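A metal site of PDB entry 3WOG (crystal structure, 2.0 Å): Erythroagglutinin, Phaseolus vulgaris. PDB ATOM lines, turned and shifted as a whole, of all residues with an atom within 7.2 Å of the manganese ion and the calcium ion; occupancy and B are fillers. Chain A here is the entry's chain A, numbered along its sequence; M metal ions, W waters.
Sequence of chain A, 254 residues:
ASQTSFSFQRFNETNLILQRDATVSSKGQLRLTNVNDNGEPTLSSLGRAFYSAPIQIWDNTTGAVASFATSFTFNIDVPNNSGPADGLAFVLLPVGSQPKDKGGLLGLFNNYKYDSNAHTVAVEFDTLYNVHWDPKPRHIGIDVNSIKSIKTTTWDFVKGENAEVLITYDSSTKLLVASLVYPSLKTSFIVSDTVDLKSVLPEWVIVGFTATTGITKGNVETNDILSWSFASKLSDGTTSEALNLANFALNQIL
Of the 26 residues printed, 4 come within 4 Å of the calcium ion.
The nearest printed residue that does not touch the calcium ion is Trp 133 (4.4 Å).
The calcium ion is bound by the side-chain amide oxygen (OD1) of Asn 130 (2.3 Å), the side-chain carboxylate (OD2) of Asp 134 (2.3 Å), water W3 (2.3 Å), the side-chain carboxylate (OD1) of Asp 126 (2.3 Å), water W1 (2.3 Å), the backbone carbonyl oxygen (O) of Leu 128 (2.4 Å) and the side-chain carboxylate (OD2) of Asp 126 (2.4 Å).
The calcium ion has seven donor atoms within binding distance.
The manganese ion is bound by water W2, water W4, NE2 of His 139, OD2 of Asp 126, OE2 of Glu 124 and OD1 of Asp 134.
N of Glu 124 sits at hydrogen-bond distance from O of Gly 141 (2.8 Å).
The side-chain carboxylate of Asp 134 sits close to the indole nitrogen of Trp 133, at 3.4 Å.
The side-chain carboxylate (OE2) of Glu 124 sits close to the side-chain hydroxyl (OG) of Ser 149, at 3.5 Å.
The backbone carbonyl oxygen (O) of Pro 137 sits at hydrogen-bond distance from a ring nitrogen (ND1) of His 139.
The side-chain carboxylate (OE1) of Glu 124 lies close to the side-chain carboxylate (OD2) of Asp 143 (2.7 Å).
Water W2 lies within hydrogen-bond range of the side-chain carboxylate of Glu 124 (2.7 Å), the backbone carbonyl oxygen of Ile 147 (3.0 Å) and the indole nitrogen of Trp 133 (3.4 Å).
Water W1 bridges O of Gly 104 and NE1 of Trp 133.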
ATOM      1  N   ASP A  86      -6.422 -16.437 -35.167  1.00  0.00           N
ATOM      2  CA  ASP A  86      -6.446 -16.407 -33.689  1.00  0.00           C
ATOM      3  C   ASP A  86      -5.067 -16.206 -33.055  1.00  0.00           C
ATOM      4  O   ASP A  86      -4.941 -15.757 -31.920  1.00  0.00           O
ATOM      5  CB  ASP A  86      -7.036 -17.700 -33.169  1.00  0.00           C
ATOM      6  CG  ASP A  86      -8.513 -17.599 -32.959  1.00  0.00           C
ATOM      7  OD1 ASP A  86      -8.925 -16.905 -31.995  1.00  0.00           O
ATOM      8  OD2 ASP A  86      -9.256 -18.203 -33.776  1.00  0.00           O
ATOM      9  N   GLY A  87      -4.033 -16.603 -33.789  1.00  0.00           N
ATOM     10  CA  GLY A  87      -2.656 -16.315 -33.385  1.00  0.00           C
ATOM     11  C   GLY A  87      -1.774 -17.518 -33.645  1.00  0.00           C
ATOM     12  O   GLY A  87      -2.188 -18.484 -34.317  1.00  0.00           O
ATOM     13  N   GLY A 103      -9.365 -22.566 -33.718  1.00  0.00           N
ATOM     14  CA  GLY A 103      -9.745 -21.249 -33.195  1.00  0.00           C
ATOM     15  C   GLY A 103      -8.923 -20.807 -32.006  1.00  0.00           C
ATOM     16  O   GLY A 103      -7.698 -20.955 -31.993  1.00  0.00           O
ATOM     17  N   GLY A 104      -9.585 -20.262 -30.987  1.00  0.00           N
ATOM     18  CA  GLY A 104      -8.883 -19.715 -29.829  1.00  0.00           C
ATOM     19  C   GLY A 104      -8.141 -20.724 -28.965  1.00  0.00           C
ATOM     20  O   GLY A 104      -7.389 -20.347 -28.083  1.00  0.00           O
ATOM     21  N   LEU A 105      -8.364 -22.012 -29.182  1.00  0.00           N
ATOM     22  CA  LEU A 105      -7.620 -23.045 -28.457  1.00  0.00           C
ATOM     23  C   LEU A 105      -6.275 -23.387 -29.122  1.00  0.00           C
ATOM     24  O   LEU A 105      -5.494 -24.212 -28.617  1.00  0.00           O
ATOM     25  CB  LEU A 105      -8.513 -24.285 -28.277  1.00  0.00           C
ATOM     26  CG  LEU A 105      -9.774 -23.988 -27.447  1.00  0.00           C
ATOM     27  CD1 LEU A 105     -10.740 -25.184 -27.383  1.00  0.00           C
ATOM     28  CD2 LEU A 105      -9.425 -23.525 -26.050  1.00  0.00           C
ATOM     29  N   LEU A 106      -6.018 -22.723 -30.250  1.00  0.00           N
ATOM     30  CA  LEU A 106      -4.708 -22.737 -30.941  1.00  0.00           C
ATOM     31  C   LEU A 106      -4.181 -24.116 -31.381  1.00  0.00           C
ATOM     32  O   LEU A 106      -2.989 -24.266 -31.629  1.00  0.00           O
ATOM     33  CB  LEU A 106      -3.642 -22.008 -30.117  1.00  0.00           C
ATOM     34  CG  LEU A 106      -3.930 -20.543 -29.768  1.00  0.00           C
ATOM     35  CD1 LEU A 106      -2.853 -19.969 -28.837  1.00  0.00           C
ATOM     36  CD2 LEU A 106      -4.048 -19.685 -31.021  1.00  0.00           C
ATOM     37  N   GLU A 124       2.500 -18.108 -26.553  1.00  0.00           N
ATOM     38  CA  GLU A 124       1.491 -17.717 -27.524  1.00  0.00           C
ATOM     39  C   GLU A 124       1.596 -16.255 -27.921  1.00  0.00           C
ATOM     40  O   GLU A 124       1.975 -15.392 -27.120  1.00  0.00           O
ATOM     41  CB  GLU A 124       0.063 -17.974 -26.968  1.00  0.00           C
ATOM     42  CG  GLU A 124      -0.336 -17.192 -25.722  1.00  0.00           C
ATOM     43  CD  GLU A 124      -1.832 -17.301 -25.414  1.00  0.00           C
ATOM     44  OE1 GLU A 124      -2.353 -18.451 -25.464  1.00  0.00           O
ATOM     45  OE2 GLU A 124      -2.510 -16.250 -25.185  1.00  0.00           O
ATOM     46  N   PHE A 125       1.217 -15.978 -29.163  1.00  0.00           N
ATOM     47  CA  PHE A 125       1.135 -14.636 -29.675  1.00  0.00           C
ATOM     48  C   PHE A 125      -0.313 -14.582 -30.130  1.00  0.00           C
ATOM     49  O   PHE A 125      -0.662 -15.082 -31.192  1.00  0.00           O
ATOM     50  CB  PHE A 125       2.189 -14.452 -30.789  1.00  0.00           C
ATOM     51  CG  PHE A 125       3.592 -14.587 -30.273  1.00  0.00           C
ATOM     52  CD1 PHE A 125       4.302 -13.484 -29.789  1.00  0.00           C
ATOM     53  CD2 PHE A 125       4.178 -15.848 -30.164  1.00  0.00           C
ATOM     54  CE1 PHE A 125       5.574 -13.626 -29.250  1.00  0.00           C
ATOM     55  CE2 PHE A 125       5.454 -15.991 -29.635  1.00  0.00           C
ATOM     56  CZ  PHE A 125       6.141 -14.887 -29.171  1.00  0.00           C
ATOM     57  N   ASP A 126      -1.149 -14.030 -29.246  1.00  0.00           N
ATOM     58  CA  ASP A 126      -2.618 -14.195 -29.293  1.00  0.00           C
ATOM     59  C   ASP A 126      -3.206 -12.898 -29.845  1.00  0.00           C
ATOM     60  O   ASP A 126      -3.054 -11.828 -29.251  1.00  0.00           O
ATOM     61  CB  ASP A 126      -3.135 -14.494 -27.840  1.00  0.00           C
ATOM     62  CG  ASP A 126      -4.617 -14.877 -27.787  1.00  0.00           C
ATOM     63  OD1 ASP A 126      -5.311 -14.594 -28.777  1.00  0.00           O
ATOM     64  OD2 ASP A 126      -5.081 -15.453 -26.724  1.00  0.00           O
ATOM     65  N   THR A 127      -3.843 -12.975 -31.016  1.00  0.00           N
ATOM     66  CA  THR A 127      -4.340 -11.762 -31.669  1.00  0.00           C
ATOM     67  C   THR A 127      -5.848 -11.569 -31.507  1.00  0.00           C
ATOM     68  O   THR A 127      -6.430 -10.662 -32.097  1.00  0.00           O
ATOM     69  CB  THR A 127      -4.058 -11.792 -33.183  1.00  0.00           C
ATOM     70  OG1 THR A 127      -4.741 -12.905 -33.753  1.00  0.00           O
ATOM     71  CG2 THR A 127      -2.529 -11.883 -33.481  1.00  0.00           C
ATOM     72  N   LEU A 128      -6.504 -12.430 -30.737  1.00  0.00           N
ATOM     73  CA  LEU A 128      -7.947 -12.289 -30.568  1.00  0.00           C
ATOM     74  C   LEU A 128      -8.379 -12.564 -29.136  1.00  0.00           C
ATOM     75  O   LEU A 128      -8.111 -13.639 -28.580  1.00  0.00           O
ATOM     76  CB  LEU A 128      -8.686 -13.207 -31.545  1.00  0.00           C
ATOM     77  CG  LEU A 128     -10.217 -13.048 -31.423  1.00  0.00           C
ATOM     78  CD1 LEU A 128     -10.844 -12.689 -32.756  1.00  0.00           C
ATOM     79  CD2 LEU A 128     -10.912 -14.213 -30.723  1.00  0.00           C
ATOM     80  N   TYR A 129      -9.041 -11.558 -28.554  1.00  0.00           N
ATOM     81  CA  TYR A 129      -9.622 -11.643 -27.221  1.00  0.00           C
ATOM     82  C   TYR A 129     -10.724 -12.703 -27.109  1.00  0.00           C
ATOM     83  O   TYR A 129     -11.773 -12.616 -27.751  1.00  0.00           O
ATOM     84  CB  TYR A 129     -10.164 -10.264 -26.820  1.00  0.00           C
ATOM     85  CG  TYR A 129     -11.071 -10.199 -25.591  1.00  0.00           C
ATOM     86  CD1 TYR A 129     -10.581 -10.510 -24.325  1.00  0.00           C
ATOM     87  CD2 TYR A 129     -12.393  -9.764 -25.707  1.00  0.00           C
ATOM     88  CE1 TYR A 129     -11.395 -10.415 -23.189  1.00  0.00           C
ATOM     89  CE2 TYR A 129     -13.225  -9.669 -24.600  1.00  0.00           C
ATOM     90  CZ  TYR A 129     -12.726  -9.988 -23.342  1.00  0.00           C
ATOM     91  OH  TYR A 129     -13.537  -9.880 -22.248  1.00  0.00           O
ATOM     92  N   ASN A 130     -10.477 -13.709 -26.284  1.00  0.00           N
ATOM     93  CA  ASN A 130     -11.460 -14.738 -26.028  1.00  0.00           C
ATOM     94  C   ASN A 130     -12.016 -14.484 -24.643  1.00  0.00           C
ATOM     95  O   ASN A 130     -11.293 -14.641 -23.634  1.00  0.00           O
ATOM     96  CB  ASN A 130     -10.822 -16.125 -26.121  1.00  0.00           C
ATOM     97  CG  ASN A 130     -10.502 -16.524 -27.542  1.00  0.00           C
ATOM     98  OD1 ASN A 130      -9.336 -16.456 -27.981  1.00  0.00           O
ATOM     99  ND2 ASN A 130     -11.528 -16.921 -28.297  1.00  0.00           N
ATOM    100  N   VAL A 131     -13.282 -14.049 -24.597  1.00  0.00           N
ATOM    101  CA  VAL A 131     -13.895 -13.532 -23.363  1.00  0.00           C
ATOM    102  C   VAL A 131     -13.751 -14.427 -22.119  1.00  0.00           C
ATOM    103  O   VAL A 131     -13.623 -13.936 -20.984  1.00  0.00           O
ATOM    104  CB  VAL A 131     -15.400 -13.189 -23.603  1.00  0.00           C
ATOM    105  CG1 VAL A 131     -16.206 -14.434 -23.959  1.00  0.00           C
ATOM    106  CG2 VAL A 131     -15.992 -12.489 -22.400  1.00  0.00           C
ATOM    107  N   TRP A 133     -11.332 -16.330 -21.163  1.00  0.00           N
ATOM    108  CA  TRP A 133     -10.009 -16.502 -20.527  1.00  0.00           C
ATOM    109  C   TRP A 133      -8.945 -15.485 -20.814  1.00  0.00           C
ATOM    110  O   TRP A 133      -7.992 -15.388 -20.046  1.00  0.00           O
ATOM    111  CB  TRP A 133      -9.449 -17.888 -20.802  1.00  0.00           C
ATOM    112  CG  TRP A 133      -9.135 -18.102 -22.265  1.00  0.00           C
ATOM    113  CD1 TRP A 133      -8.012 -17.668 -22.971  1.00  0.00           C
ATOM    114  CD2 TRP A 133      -9.962 -18.796 -23.242  1.00  0.00           C
ATOM    115  NE1 TRP A 133      -8.091 -18.052 -24.294  1.00  0.00           N
ATOM    116  CE2 TRP A 133      -9.234 -18.733 -24.526  1.00  0.00           C
ATOM    117  CE3 TRP A 133     -11.191 -19.462 -23.206  1.00  0.00           C
ATOM    118  CZ2 TRP A 133      -9.740 -19.304 -25.680  1.00  0.00           C
ATOM    119  CZ3 TRP A 133     -11.679 -20.042 -24.385  1.00  0.00           C
ATOM    120  CH2 TRP A 133     -10.965 -19.969 -25.578  1.00  0.00           C
ATOM    121  N   ASP A 134      -9.042 -14.746 -21.926  1.00  0.00           N
ATOM    122  CA  ASP A 134      -7.952 -13.831 -22.329  1.00  0.00           C
ATOM    123  C   ASP A 134      -7.998 -12.480 -21.629  1.00  0.00           C
ATOM    124  O   ASP A 134      -9.090 -11.993 -21.288  1.00  0.00           O
ATOM    125  CB  ASP A 134      -8.012 -13.560 -23.829  1.00  0.00           C
ATOM    126  CG  ASP A 134      -7.295 -14.629 -24.667  1.00  0.00           C
ATOM    127  OD1 ASP A 134      -6.223 -15.209 -24.269  1.00  0.00           O
ATOM    128  OD2 ASP A 134      -7.825 -14.851 -25.779  1.00  0.00           O
ATOM    129  N   PRO A 135      -6.820 -11.830 -21.448  1.00  0.00           N
ATOM    130  CA  PRO A 135      -6.870 -10.386 -21.217  1.00  0.00           C
ATOM    131  C   PRO A 135      -7.352  -9.679 -22.494  1.00  0.00           C
ATOM    132  O   PRO A 135      -7.173 -10.201 -23.600  1.00  0.00           O
ATOM    133  CB  PRO A 135      -5.408 -10.004 -20.901  1.00  0.00           C
ATOM    134  CG  PRO A 135      -4.570 -11.132 -21.440  1.00  0.00           C
ATOM    135  CD  PRO A 135      -5.438 -12.362 -21.509  1.00  0.00           C
ATOM    136  N   PRO A 137      -6.460  -6.726 -24.159  1.00  0.00           N
ATOM    137  CA  PRO A 137      -5.490  -6.353 -25.195  1.00  0.00           C
ATOM    138  C   PRO A 137      -4.851  -7.613 -25.821  1.00  0.00           C
ATOM    139  O   PRO A 137      -4.740  -8.643 -25.157  1.00  0.00           O
ATOM    140  CB  PRO A 137      -4.425  -5.575 -24.417  1.00  0.00           C
ATOM    141  CG  PRO A 137      -5.067  -5.210 -23.092  1.00  0.00           C
ATOM    142  CD  PRO A 137      -5.996  -6.348 -22.810  1.00  0.00           C
ATOM    143  N   HIS A 139      -1.754  -9.912 -26.832  1.00  0.00           N
ATOM    144  CA  HIS A 139      -0.830 -10.270 -25.757  1.00  0.00           C
ATOM    145  C   HIS A 139       0.150 -11.353 -26.133  1.00  0.00           C
ATOM    146  O   HIS A 139      -0.134 -12.172 -26.995  1.00  0.00           O
ATOM    147  CB  HIS A 139      -1.622 -10.677 -24.487  1.00  0.00           C
ATOM    148  CG  HIS A 139      -2.633 -11.811 -24.702  1.00  0.00           C
ATOM    149  ND1 HIS A 139      -3.878 -11.597 -25.147  1.00  0.00           N
ATOM    150  CD2 HIS A 139      -2.531 -13.193 -24.450  1.00  0.00           C
ATOM    151  CE1 HIS A 139      -4.549 -12.761 -25.224  1.00  0.00           C
ATOM    152  NE2 HIS A 139      -3.723 -13.753 -24.792  1.00  0.00           N
ATOM    153  N   ILE A 140       1.327 -11.326 -25.509  1.00  0.00           N
ATOM    154  CA  ILE A 140       2.219 -12.491 -25.507  1.00  0.00           C
ATOM    155  C   ILE A 140       1.898 -13.213 -24.209  1.00  0.00           C
ATOM    156  O   ILE A 140       1.781 -12.569 -23.167  1.00  0.00           O
ATOM    157  CB  ILE A 140       3.718 -12.088 -25.543  1.00  0.00           C
ATOM    158  CG1 ILE A 140       3.995 -11.135 -26.706  1.00  0.00           C
ATOM    159  CG2 ILE A 140       4.604 -13.331 -25.628  1.00  0.00           C
ATOM    160  CD1 ILE A 140       5.372 -10.490 -26.660  1.00  0.00           C
ATOM    161  N   GLY A 141       1.681 -14.527 -24.292  1.00  0.00           N
ATOM    162  CA  GLY A 141       1.383 -15.337 -23.100  1.00  0.00           C
ATOM    163  C   GLY A 141       2.250 -16.597 -22.932  1.00  0.00           C
ATOM    164  O   GLY A 141       2.629 -17.233 -23.922  1.00  0.00           O
ATOM    165  N   ASP A 143       1.987 -20.296 -21.623  1.00  0.00           N
ATOM    166  CA  ASP A 143       0.935 -21.272 -21.397  1.00  0.00           C
ATOM    167  C   ASP A 143       1.543 -22.549 -20.837  1.00  0.00           C
ATOM    168  O   ASP A 143       2.507 -23.082 -21.411  1.00  0.00           O
ATOM    169  CB  ASP A 143       0.191 -21.650 -22.697  1.00  0.00           C
ATOM    170  CG  ASP A 143      -0.514 -20.462 -23.347  1.00  0.00           C
ATOM    171  OD1 ASP A 143      -0.583 -19.380 -22.734  1.00  0.00           O
ATOM    172  OD2 ASP A 143      -1.030 -20.629 -24.487  1.00  0.00           O
ATOM    173  N   ILE A 147      -4.977 -23.015 -22.001  1.00  0.00           N
ATOM    174  CA  ILE A 147      -5.102 -21.846 -22.880  1.00  0.00           C
ATOM    175  C   ILE A 147      -5.140 -20.551 -22.057  1.00  0.00           C
ATOM    176  O   ILE A 147      -4.916 -19.444 -22.578  1.00  0.00           O
ATOM    177  CB  ILE A 147      -6.340 -21.973 -23.817  1.00  0.00           C
ATOM    178  CG1 ILE A 147      -6.210 -21.099 -25.079  1.00  0.00           C
ATOM    179  CG2 ILE A 147      -7.637 -21.654 -23.066  1.00  0.00           C
ATOM    180  CD1 ILE A 147      -4.940 -21.326 -25.886  1.00  0.00           C
ATOM    181  N   LYS A 148      -5.392 -20.695 -20.751  1.00  0.00           N
ATOM    182  CA  LYS A 148      -5.389 -19.549 -19.874  1.00  0.00           C
ATOM    183  C   LYS A 148      -3.968 -19.318 -19.396  1.00  0.00           C
ATOM    184  O   LYS A 148      -3.499 -20.016 -18.503  1.00  0.00           O
ATOM    185  CB  LYS A 148      -6.339 -19.723 -18.676  1.00  0.00           C
ATOM    186  CG  LYS A 148      -6.483 -18.443 -17.873  1.00  0.00           C
ATOM    187  CD  LYS A 148      -7.134 -18.630 -16.511  1.00  0.00           C
ATOM    188  CE  LYS A 148      -6.647 -17.509 -15.588  1.00  0.00           C
ATOM    189  NZ  LYS A 148      -7.341 -17.411 -14.275  1.00  0.00           N
ATOM    190  N   SER A 149      -3.287 -18.328 -19.988  1.00  0.00           N
ATOM    191  CA  SER A 149      -1.860 -18.108 -19.734  1.00  0.00           C
ATOM    192  C   SER A 149      -1.559 -17.875 -18.262  1.00  0.00           C
ATOM    193  O   SER A 149      -2.324 -17.195 -17.559  1.00  0.00           O
ATOM    194  CB  SER A 149      -1.326 -16.937 -20.564  1.00  0.00           C
ATOM    195  OG  SER A 149      -1.721 -17.071 -21.926  1.00  0.00           O
ATOM    196  N   THR A 152       0.966 -12.980 -18.875  1.00  0.00           N
ATOM    197  CA  THR A 152       0.807 -12.290 -20.161  1.00  0.00           C
ATOM    198  C   THR A 152       1.435 -10.891 -20.120  1.00  0.00           C
ATOM    199  O   THR A 152       1.683 -10.336 -19.048  1.00  0.00           O
ATOM    200  CB  THR A 152      -0.673 -12.127 -20.580  1.00  0.00           C
ATOM    201  OG1 THR A 152      -1.359 -11.355 -19.589  1.00  0.00           O
ATOM    202  CG2 THR A 152      -1.367 -13.481 -20.714  1.00  0.00           C
HETATM  203 MN    MN M   1      -4.369 -15.619 -24.878  1.00  0.00          MN
HETATM  204 CA    CA M   2      -7.164 -15.667 -27.846  1.00  0.00          CA
HETATM  205  O   HOH W   1      -6.679 -17.789 -26.982  1.00  0.00           O
HETATM  206  O   HOH W   2      -4.803 -17.507 -24.812  1.00  0.00           O
HETATM  207  O   HOH W   3      -7.144 -16.395 -30.055  1.00  0.00           O
HETATM  208  O   HOH W   4      -3.866 -15.801 -23.008  1.00  0.00           O
